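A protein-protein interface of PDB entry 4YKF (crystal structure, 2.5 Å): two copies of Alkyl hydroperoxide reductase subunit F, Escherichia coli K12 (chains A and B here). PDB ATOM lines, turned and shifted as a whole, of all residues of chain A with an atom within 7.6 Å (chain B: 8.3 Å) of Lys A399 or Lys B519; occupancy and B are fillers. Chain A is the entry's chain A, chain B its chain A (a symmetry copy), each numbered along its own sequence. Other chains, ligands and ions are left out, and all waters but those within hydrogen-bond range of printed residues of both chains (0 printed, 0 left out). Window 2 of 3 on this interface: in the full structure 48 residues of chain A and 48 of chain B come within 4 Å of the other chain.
The backbone carbonyl oxygen (O) of Lys A399 is in hydrogen-bond range of the side-chain hydroxyl (OG) of Ser A402 (2.7 Å).
NE of Arg B517 is in salt-bridge range of OD1 of Asp B513, at 3.1 Å.
Hydrophobic or aromatic side chains of chain B that line the printed part of chain A: Ile B516.
Printed residues of chain A that touch a printed residue of chain B: Ile A372, Asp A393, Val A395, Leu A396 and Lys A399.
Hydrophobic or aromatic side chains of chain A within 4 Å of the printed part of chain B: Ile A372, Val A395 and Leu A396.
Among the printed residues, Asp or Glu carboxylates within 4 Å of a Lys or Arg side-chain nitrogen of the other chain: Asp A393 with Arg B517 (2.9 Å).
Printed residues of chain B within 4 Å of Ile A372: Ile B516 (3.8 Å).
Printed residues of chain B within 4 Å of Val A395: Arg B517 (3.9 Å).
Printed residues of chain B within 4 Å of Leu A396: Arg B517 (3.8 Å).
Lys A399 touches just these residues of chain B: Ile B516 (3.4 Å) and Lys B519 (3.6 Å).
Of the printed residues of chain A, Ile B516 touches Ile A372 and Lys A399.
Printed residues of chain A within 4 Å of Lys B519: Lys A399.
Thr B520 touches none of the printed residues of chain A.
The nearest residue of chain B that does not touch Lys A399 is Leu B515 (4.9 Å).
The nearest residue of chain A that does not touch Lys B519 is Val A395 (7.1 Å).
The nearest printed residue of chain A that does not touch Ile B516 is Leu A396 (4.1 Å).
Ile B516 touches Ile A372 (CG2 to CG2, 3.8 Å).
Val A395 touches Arg B517.
Arg B517 touches Leu A396.
Ile B516 touches Lys A399 (O to CG, 3.4 Å).
Lys B519 touches Lys A399 (CG to NZ, 3.6 Å).
No position is printed for both chains.
Of the 6 pairs that touch across the chains among the printed residues, none has its exchanged pair printed and touching as well.
The side-chain carboxylate (OD2) of Asp A393 is in salt-bridge range of the guanidinium group (NH2) of Arg B517 (2.9 Å).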
ATOM      1  N   VAL A 368      17.002   3.500  15.064  1.00  0.00           N
ATOM      2  CA  VAL A 368      15.763   3.395  15.772  1.00  0.00           C
ATOM      3  C   VAL A 368      14.699   4.298  15.130  1.00  0.00           C
ATOM      4  O   VAL A 368      13.593   3.861  14.881  1.00  0.00           O
ATOM      5  CB  VAL A 368      15.934   3.697  17.260  1.00  0.00           C
ATOM      6  CG1 VAL A 368      14.595   3.508  17.985  1.00  0.00           C
ATOM      7  CG2 VAL A 368      16.937   2.737  17.841  1.00  0.00           C
ATOM      8  N   ILE A 372      11.022   2.856  13.256  1.00  0.00           N
ATOM      9  CA  ILE A 372       9.690   3.330  13.515  1.00  0.00           C
ATOM     10  C   ILE A 372       9.099   3.860  12.206  1.00  0.00           C
ATOM     11  O   ILE A 372       7.985   3.486  11.825  1.00  0.00           O
ATOM     12  CB  ILE A 372       9.711   4.442  14.586  1.00  0.00           C
ATOM     13  CG1 ILE A 372      10.431   3.954  15.871  1.00  0.00           C
ATOM     14  CG2 ILE A 372       8.278   4.886  14.908  1.00  0.00           C
ATOM     15  CD1 ILE A 372      11.010   5.065  16.727  1.00  0.00           C
ATOM     16  N   ALA A 375       8.479   0.710  10.050  1.00  0.00           N
ATOM     17  CA  ALA A 375       7.354   0.030  10.680  1.00  0.00           C
ATOM     18  C   ALA A 375       5.976   0.532  10.203  1.00  0.00           C
ATOM     19  O   ALA A 375       5.066  -0.240  10.024  1.00  0.00           O
ATOM     20  CB  ALA A 375       7.457   0.182  12.180  1.00  0.00           C
ATOM     21  N   ASP A 393      17.996   7.206  22.299  1.00  0.00           N
ATOM     22  CA  ASP A 393      17.173   7.865  23.330  1.00  0.00           C
ATOM     23  C   ASP A 393      16.137   6.881  23.779  1.00  0.00           C
ATOM     24  O   ASP A 393      15.461   6.301  22.940  1.00  0.00           O
ATOM     25  CB  ASP A 393      16.384   9.082  22.780  1.00  0.00           C
ATOM     26  CG  ASP A 393      17.262  10.264  22.403  1.00  0.00           C
ATOM     27  OD1 ASP A 393      18.343  10.387  22.976  1.00  0.00           O
ATOM     28  OD2 ASP A 393      16.858  11.078  21.526  1.00  0.00           O
ATOM     29  N   GLN A 394      16.019   6.715  25.096  1.00  0.00           N
ATOM     30  CA  GLN A 394      15.080   5.810  25.728  1.00  0.00           C
ATOM     31  C   GLN A 394      13.686   5.929  25.174  1.00  0.00           C
ATOM     32  O   GLN A 394      12.963   4.922  25.029  1.00  0.00           O
ATOM     33  CB  GLN A 394      15.020   6.075  27.248  1.00  0.00           C
ATOM     34  CG  GLN A 394      15.616   4.938  28.089  1.00  0.00           C
ATOM     35  CD  GLN A 394      14.864   3.651  27.857  1.00  0.00           C
ATOM     36  OE1 GLN A 394      13.635   3.627  28.006  1.00  0.00           O
ATOM     37  NE2 GLN A 394      15.569   2.591  27.442  1.00  0.00           N
ATOM     38  N   VAL A 395      13.292   7.164  24.882  1.00  0.00           N
ATOM     39  CA  VAL A 395      11.899   7.446  24.535  1.00  0.00           C
ATOM     40  C   VAL A 395      11.656   6.860  23.112  1.00  0.00           C
ATOM     41  O   VAL A 395      10.576   6.382  22.781  1.00  0.00           O
ATOM     42  CB  VAL A 395      11.562   8.962  24.687  1.00  0.00           C
ATOM     43  CG1 VAL A 395      12.703   9.715  25.388  1.00  0.00           C
ATOM     44  CG2 VAL A 395      11.289   9.627  23.358  1.00  0.00           C
ATOM     45  N   LEU A 396      12.693   6.850  22.296  1.00  0.00           N
ATOM     46  CA  LEU A 396      12.617   6.140  21.036  1.00  0.00           C
ATOM     47  C   LEU A 396      12.614   4.631  21.218  1.00  0.00           C
ATOM     48  O   LEU A 396      11.889   3.955  20.495  1.00  0.00           O
ATOM     49  CB  LEU A 396      13.742   6.553  20.102  1.00  0.00           C
ATOM     50  CG  LEU A 396      13.681   8.018  19.699  1.00  0.00           C
ATOM     51  CD1 LEU A 396      14.898   8.295  18.867  1.00  0.00           C
ATOM     52  CD2 LEU A 396      12.428   8.364  18.922  1.00  0.00           C
ATOM     53  N   GLN A 397      13.389   4.100  22.172  1.00  0.00           N
ATOM     54  CA  GLN A 397      13.411   2.635  22.399  1.00  0.00           C
ATOM     55  C   GLN A 397      12.042   2.147  22.783  1.00  0.00           C
ATOM     56  O   GLN A 397      11.501   1.286  22.140  1.00  0.00           O
ATOM     57  CB  GLN A 397      14.441   2.199  23.462  1.00  0.00           C
ATOM     58  CG  GLN A 397      15.901   2.318  23.020  1.00  0.00           C
ATOM     59  CD  GLN A 397      16.892   1.752  24.024  1.00  0.00           C
ATOM     60  OE1 GLN A 397      16.768   0.625  24.471  1.00  0.00           O
ATOM     61  NE2 GLN A 397      17.912   2.529  24.342  1.00  0.00           N
ATOM     62  N   ASP A 398      11.475   2.736  23.827  1.00  0.00           N
ATOM     63  CA  ASP A 398      10.099   2.425  24.278  1.00  0.00           C
ATOM     64  C   ASP A 398       9.144   2.377  23.120  1.00  0.00           C
ATOM     65  O   ASP A 398       8.540   1.347  22.878  1.00  0.00           O
ATOM     66  CB  ASP A 398       9.627   3.443  25.307  1.00  0.00           C
ATOM     67  CG  ASP A 398      10.619   3.598  26.461  1.00  0.00           C
ATOM     68  OD1 ASP A 398      11.403   2.626  26.689  1.00  0.00           O
ATOM     69  OD2 ASP A 398      10.630   4.696  27.107  1.00  0.00           O
ATOM     70  N   LYS A 399       9.096   3.471  22.363  1.00  0.00           N
ATOM     71  CA  LYS A 399       8.279   3.598  21.126  1.00  0.00           C
ATOM     72  C   LYS A 399       8.498   2.493  20.069  1.00  0.00           C
ATOM     73  O   LYS A 399       7.557   1.999  19.471  1.00  0.00           O
ATOM     74  CB  LYS A 399       8.510   4.980  20.480  1.00  0.00           C
ATOM     75  CG  LYS A 399       7.610   5.315  19.260  1.00  0.00           C
ATOM     76  CD  LYS A 399       6.121   5.431  19.629  1.00  0.00           C
ATOM     77  CE  LYS A 399       5.188   5.407  18.427  1.00  0.00           C
ATOM     78  NZ  LYS A 399       3.902   6.121  18.742  1.00  0.00           N
ATOM     79  N   LEU A 400       9.741   2.121  19.828  1.00  0.00           N
ATOM     80  CA  LEU A 400      10.033   1.000  18.942  1.00  0.00           C
ATOM     81  C   LEU A 400       9.669  -0.332  19.596  1.00  0.00           C
ATOM     82  O   LEU A 400       9.217  -1.234  18.914  1.00  0.00           O
ATOM     83  CB  LEU A 400      11.508   1.004  18.512  1.00  0.00           C
ATOM     84  CG  LEU A 400      11.897  -0.077  17.482  1.00  0.00           C
ATOM     85  CD1 LEU A 400      11.284   0.194  16.113  1.00  0.00           C
ATOM     86  CD2 LEU A 400      13.401  -0.272  17.370  1.00  0.00           C
ATOM     87  N   ARG A 401       9.855  -0.469  20.906  1.00  0.00           N
ATOM     88  CA  ARG A 401       9.444  -1.710  21.590  1.00  0.00           C
ATOM     89  C   ARG A 401       7.933  -1.748  21.689  1.00  0.00           C
ATOM     90  O   ARG A 401       7.367  -2.775  21.924  1.00  0.00           O
ATOM     91  CB  ARG A 401      10.075  -1.883  22.988  1.00  0.00           C
ATOM     92  CG  ARG A 401      11.590  -2.116  22.975  1.00  0.00           C
ATOM     93  CD  ARG A 401      12.180  -2.103  24.382  1.00  0.00           C
ATOM     94  NE  ARG A 401      13.635  -2.322  24.419  1.00  0.00           N
ATOM     95  CZ  ARG A 401      14.235  -3.501  24.219  1.00  0.00           C
ATOM     96  NH1 ARG A 401      13.514  -4.594  23.934  1.00  0.00           N
ATOM     97  NH2 ARG A 401      15.573  -3.588  24.263  1.00  0.00           N
ATOM     98  N   SER A 402       7.257  -0.642  21.461  1.00  0.00           N
ATOM     99  CA  SER A 402       5.806  -0.687  21.550  1.00  0.00           C
ATOM    100  C   SER A 402       5.212  -1.388  20.344  1.00  0.00           C
ATOM    101  O   SER A 402       4.152  -1.965  20.469  1.00  0.00           O
ATOM    102  CB  SER A 402       5.194   0.706  21.700  1.00  0.00           C
ATOM    103  OG  SER A 402       5.084   1.346  20.436  1.00  0.00           O
ATOM    104  N   LEU A 403       5.875  -1.375  19.184  1.00  0.00           N
ATOM    105  CA  LEU A 403       5.170  -1.761  17.959  1.00  0.00           C
ATOM    106  C   LEU A 403       5.005  -3.270  17.796  1.00  0.00           C
ATOM    107  O   LEU A 403       5.671  -4.056  18.475  1.00  0.00           O
ATOM    108  CB  LEU A 403       5.827  -1.136  16.736  1.00  0.00           C
ATOM    109  CG  LEU A 403       5.892   0.400  16.794  1.00  0.00           C
ATOM    110  CD1 LEU A 403       6.560   0.998  15.563  1.00  0.00           C
ATOM    111  CD2 LEU A 403       4.514   0.983  16.974  1.00  0.00           C
ATOM    112  N   LYS A 404       4.098  -3.678  16.912  1.00  0.00           N
ATOM    113  CA  LYS A 404       3.749  -5.092  16.828  1.00  0.00           C
ATOM    114  C   LYS A 404       4.290  -5.827  15.606  1.00  0.00           C
ATOM    115  O   LYS A 404       4.000  -6.984  15.430  1.00  0.00           O
ATOM    116  CB  LYS A 404       2.220  -5.238  16.945  1.00  0.00           C
ATOM    117  CG  LYS A 404       1.714  -4.868  18.350  1.00  0.00           C
ATOM    118  CD  LYS A 404       0.270  -5.269  18.582  1.00  0.00           C
ATOM    119  CE  LYS A 404      -0.643  -4.560  17.590  1.00  0.00           C
ATOM    120  NZ  LYS A 404      -2.074  -4.688  17.967  1.00  0.00           N
ATOM    121  N   VAL A 406       7.754  -5.414  14.719  1.00  0.00           N
ATOM    122  CA  VAL A 406       9.174  -5.143  14.821  1.00  0.00           C
ATOM    123  C   VAL A 406       9.823  -6.182  15.689  1.00  0.00           C
ATOM    124  O   VAL A 406       9.228  -6.628  16.653  1.00  0.00           O
ATOM    125  CB  VAL A 406       9.450  -3.813  15.508  1.00  0.00           C
ATOM    126  CG1 VAL A 406      10.933  -3.653  15.747  1.00  0.00           C
ATOM    127  CG2 VAL A 406       8.927  -2.651  14.673  1.00  0.00           C
ATOM    128  N   ASP B 214      -2.558  13.827  11.217  1.00  0.00           N
ATOM    129  CA  ASP B 214      -1.236  13.665  11.834  1.00  0.00           C
ATOM    130  C   ASP B 214      -0.458  14.959  11.618  1.00  0.00           C
ATOM    131  O   ASP B 214       0.171  15.477  12.540  1.00  0.00           O
ATOM    132  CB  ASP B 214      -0.470  12.458  11.274  1.00  0.00           C
ATOM    133  CG  ASP B 214      -1.112  11.117  11.655  1.00  0.00           C
ATOM    134  OD1 ASP B 214      -1.476  10.937  12.820  1.00  0.00           O
ATOM    135  OD2 ASP B 214      -1.230  10.232  10.769  1.00  0.00           O
ATOM    136  N   ILE B 236       1.808   9.045   6.813  1.00  0.00           N
ATOM    137  CA  ILE B 236       0.977   9.552   7.866  1.00  0.00           C
ATOM    138  C   ILE B 236      -0.150  10.347   7.223  1.00  0.00           C
ATOM    139  O   ILE B 236      -0.090  10.709   6.074  1.00  0.00           O
ATOM    140  CB  ILE B 236       1.737  10.435   8.853  1.00  0.00           C
ATOM    141  CG1 ILE B 236       2.089  11.757   8.183  1.00  0.00           C
ATOM    142  CG2 ILE B 236       2.952   9.702   9.410  1.00  0.00           C
ATOM    143  CD1 ILE B 236       3.186  12.502   8.880  1.00  0.00           C
ATOM    144  N   GLU B 299       0.517  18.285  25.988  1.00  0.00           N
ATOM    145  CA  GLU B 299       1.582  17.648  25.249  1.00  0.00           C
ATOM    146  C   GLU B 299       1.237  16.457  24.382  1.00  0.00           C
ATOM    147  O   GLU B 299       2.021  16.142  23.504  1.00  0.00           O
ATOM    148  CB  GLU B 299       2.728  17.272  26.201  1.00  0.00           C
ATOM    149  CG  GLU B 299       2.310  16.602  27.514  1.00  0.00           C
ATOM    150  CD  GLU B 299       1.874  17.571  28.629  1.00  0.00           C
ATOM    151  OE1 GLU B 299       1.688  18.799  28.393  1.00  0.00           O
ATOM    152  OE2 GLU B 299       1.692  17.079  29.764  1.00  0.00           O
ATOM    153  N   GLY B 300       0.103  15.795  24.584  1.00  0.00           N
ATOM    154  CA  GLY B 300      -0.379  14.832  23.562  1.00  0.00           C
ATOM    155  C   GLY B 300      -1.668  15.252  22.838  1.00  0.00           C
ATOM    156  O   GLY B 300      -2.401  14.412  22.277  1.00  0.00           O
ATOM    157  N   GLY B 301      -1.955  16.547  22.839  1.00  0.00           N
ATOM    158  CA  GLY B 301      -3.278  16.997  22.451  1.00  0.00           C
ATOM    159  C   GLY B 301      -3.457  17.133  20.958  1.00  0.00           C
ATOM    160  O   GLY B 301      -2.880  16.378  20.170  1.00  0.00           O
ATOM    161  N   ARG B 316      -2.268  16.677  15.060  1.00  0.00           N
ATOM    162  CA  ARG B 316      -1.227  16.448  16.065  1.00  0.00           C
ATOM    163  C   ARG B 316      -0.042  17.357  15.820  1.00  0.00           C
ATOM    164  O   ARG B 316       0.720  17.608  16.728  1.00  0.00           O
ATOM    165  CB  ARG B 316      -0.689  15.013  16.037  1.00  0.00           C
ATOM    166  CG  ARG B 316      -1.701  13.885  16.248  1.00  0.00           C
ATOM    167  CD  ARG B 316      -0.946  12.582  16.544  1.00  0.00           C
ATOM    168  NE  ARG B 316      -1.780  11.384  16.401  1.00  0.00           N
ATOM    169  CZ  ARG B 316      -2.322  10.673  17.394  1.00  0.00           C
ATOM    170  NH1 ARG B 316      -2.175  11.012  18.662  1.00  0.00           N
ATOM    171  NH2 ARG B 316      -3.058   9.600  17.099  1.00  0.00           N
ATOM    172  N   PHE B 512       7.621  14.877  11.760  1.00  0.00           N
ATOM    173  CA  PHE B 512       7.522  13.454  11.900  1.00  0.00           C
ATOM    174  C   PHE B 512       8.272  13.052  13.172  1.00  0.00           C
ATOM    175  O   PHE B 512       7.771  12.255  13.942  1.00  0.00           O
ATOM    176  CB  PHE B 512       8.068  12.728  10.688  1.00  0.00           C
ATOM    177  CG  PHE B 512       8.093  11.248  10.839  1.00  0.00           C
ATOM    178  CD1 PHE B 512       6.924  10.497  10.633  1.00  0.00           C
ATOM    179  CD2 PHE B 512       9.266  10.581  11.160  1.00  0.00           C
ATOM    180  CE1 PHE B 512       6.917   9.113  10.767  1.00  0.00           C
ATOM    181  CE2 PHE B 512       9.273   9.198  11.274  1.00  0.00           C
ATOM    182  CZ  PHE B 512       8.090   8.465  11.083  1.00  0.00           C
ATOM    183  N   ASP B 513       9.432  13.648  13.392  1.00  0.00           N
ATOM    184  CA  ASP B 513      10.264  13.287  14.509  1.00  0.00           C
ATOM    185  C   ASP B 513       9.561  13.608  15.815  1.00  0.00           C
ATOM    186  O   ASP B 513       9.691  12.906  16.825  1.00  0.00           O
ATOM    187  CB  ASP B 513      11.600  13.985  14.442  1.00  0.00           C
ATOM    188  CG  ASP B 513      12.368  13.893  15.772  1.00  0.00           C
ATOM    189  OD1 ASP B 513      13.164  12.943  15.984  1.00  0.00           O
ATOM    190  OD2 ASP B 513      12.160  14.758  16.654  1.00  0.00           O
ATOM    191  N   TYR B 514       8.759  14.653  15.775  1.00  0.00           N
ATOM    192  CA  TYR B 514       7.957  15.047  16.909  1.00  0.00           C
ATOM    193  C   TYR B 514       6.881  14.066  17.137  1.00  0.00           C
ATOM    194  O   TYR B 514       6.619  13.744  18.253  1.00  0.00           O
ATOM    195  CB  TYR B 514       7.360  16.452  16.660  1.00  0.00           C
ATOM    196  CG  TYR B 514       6.322  16.872  17.654  1.00  0.00           C
ATOM    197  CD1 TYR B 514       6.665  17.524  18.816  1.00  0.00           C
ATOM    198  CD2 TYR B 514       4.971  16.604  17.411  1.00  0.00           C
ATOM    199  CE1 TYR B 514       5.704  17.879  19.737  1.00  0.00           C
ATOM    200  CE2 TYR B 514       4.007  16.963  18.321  1.00  0.00           C
ATOM    201  CZ  TYR B 514       4.397  17.604  19.478  1.00  0.00           C
ATOM    202  OH  TYR B 514       3.435  17.963  20.340  1.00  0.00           O
ATOM    203  N   LEU B 515       6.197  13.632  16.111  1.00  0.00           N
ATOM    204  CA  LEU B 515       5.121  12.686  16.327  1.00  0.00           C
ATOM    205  C   LEU B 515       5.616  11.405  16.966  1.00  0.00           C
ATOM    206  O   LEU B 515       4.965  10.844  17.794  1.00  0.00           O
ATOM    207  CB  LEU B 515       4.444  12.295  15.036  1.00  0.00           C
ATOM    208  CG  LEU B 515       3.457  13.324  14.529  1.00  0.00           C
ATOM    209  CD1 LEU B 515       3.194  13.138  13.037  1.00  0.00           C
ATOM    210  CD2 LEU B 515       2.195  13.165  15.335  1.00  0.00           C
ATOM    211  N   ILE B 516       6.760  10.918  16.568  1.00  0.00           N
ATOM    212  CA  ILE B 516       7.114   9.606  17.015  1.00  0.00           C
ATOM    213  C   ILE B 516       7.685   9.646  18.448  1.00  0.00           C
ATOM    214  O   ILE B 516       7.623   8.671  19.196  1.00  0.00           O
ATOM    215  CB  ILE B 516       8.067   8.932  16.016  1.00  0.00           C
ATOM    216  CG1 ILE B 516       9.256   9.846  15.734  1.00  0.00           C
ATOM    217  CG2 ILE B 516       7.350   8.576  14.726  1.00  0.00           C
ATOM    218  CD1 ILE B 516      10.515   9.088  15.396  1.00  0.00           C
ATOM    219  N   ARG B 517       8.226  10.798  18.808  1.00  0.00           N
ATOM    220  CA  ARG B 517       8.797  11.048  20.126  1.00  0.00           C
ATOM    221  C   ARG B 517       7.708  11.313  21.147  1.00  0.00           C
ATOM    222  O   ARG B 517       7.924  11.269  22.346  1.00  0.00           O
ATOM    223  CB  ARG B 517       9.685  12.282  20.072  1.00  0.00           C
ATOM    224  CG  ARG B 517      11.100  11.967  19.680  1.00  0.00           C
ATOM    225  CD  ARG B 517      11.925  13.229  19.529  1.00  0.00           C
ATOM    226  NE  ARG B 517      13.253  12.865  19.040  1.00  0.00           N
ATOM    227  CZ  ARG B 517      14.224  12.357  19.792  1.00  0.00           C
ATOM    228  NH1 ARG B 517      14.031  12.136  21.085  1.00  0.00           N
ATOM    229  NH2 ARG B 517      15.401  12.064  19.236  1.00  0.00           N
ATOM    230  N   THR B 518       6.543  11.647  20.665  1.00  0.00           N
ATOM    231  CA  THR B 518       5.526  12.089  21.537  1.00  0.00           C
ATOM    232  C   THR B 518       4.452  11.090  21.327  1.00  0.00           C
ATOM    233  O   THR B 518       3.794  11.092  20.278  1.00  0.00           O
ATOM    234  CB  THR B 518       5.019  13.503  21.159  1.00  0.00           C
ATOM    235  OG1 THR B 518       4.285  13.434  19.923  1.00  0.00           O
ATOM    236  CG2 THR B 518       6.228  14.555  21.069  1.00  0.00           C
ATOM    237  N   LYS B 519       4.326  10.186  22.291  1.00  0.00           N
ATOM    238  CA  LYS B 519       3.078   9.459  22.451  1.00  0.00           C
ATOM    239  C   LYS B 519       2.885   9.063  23.921  1.00  0.00           C
ATOM    240  O   LYS B 519       1.983   9.581  24.556  1.00  0.00           O
ATOM    241  CB  LYS B 519       2.992   8.265  21.482  1.00  0.00           C
ATOM    242  CG  LYS B 519       1.734   8.246  20.597  1.00  0.00           C
ATOM    243  CD  LYS B 519       1.877   9.138  19.361  1.00  0.00           C
ATOM    244  CE  LYS B 519       1.005   8.695  18.192  1.00  0.00           C
ATOM    245  NZ  LYS B 519       1.480   9.319  16.918  1.00  0.00           N
ATOM    246  N   THR B 520       3.743   8.183  24.440  1.00  0.00           N
ATOM    247  CA  THR B 520       3.614   7.609  25.787  1.00  0.00           C
ATOM    248  C   THR B 520       2.266   6.900  26.015  1.00  0.00           C
ATOM    249  O   THR B 520       1.562   7.157  27.005  1.00  0.00           O
ATOM    250  CB  THR B 520       3.805   8.677  26.896  1.00  0.00           C
ATOM    251  OG1 THR B 520       4.750   9.675  26.463  1.00  0.00           O
ATOM    252  CG2 THR B 520       4.250   8.004  28.241  1.00  0.00           C
ATOM    253  N   ALA B 521       1.899   6.016  25.099  1.00  0.00           N
ATOM    254  CA  ALA B 521       0.614   5.322  25.219  1.00  0.00           C
ATOM    255  C   ALA B 521      -0.513   6.330  25.421  1.00  0.00           C
ATOM    256  O   ALA B 521      -1.660   5.942  25.615  1.00  0.00           O
ATOM    257  CB  ALA B 521       0.645   4.317  26.376  1.00  0.00           C
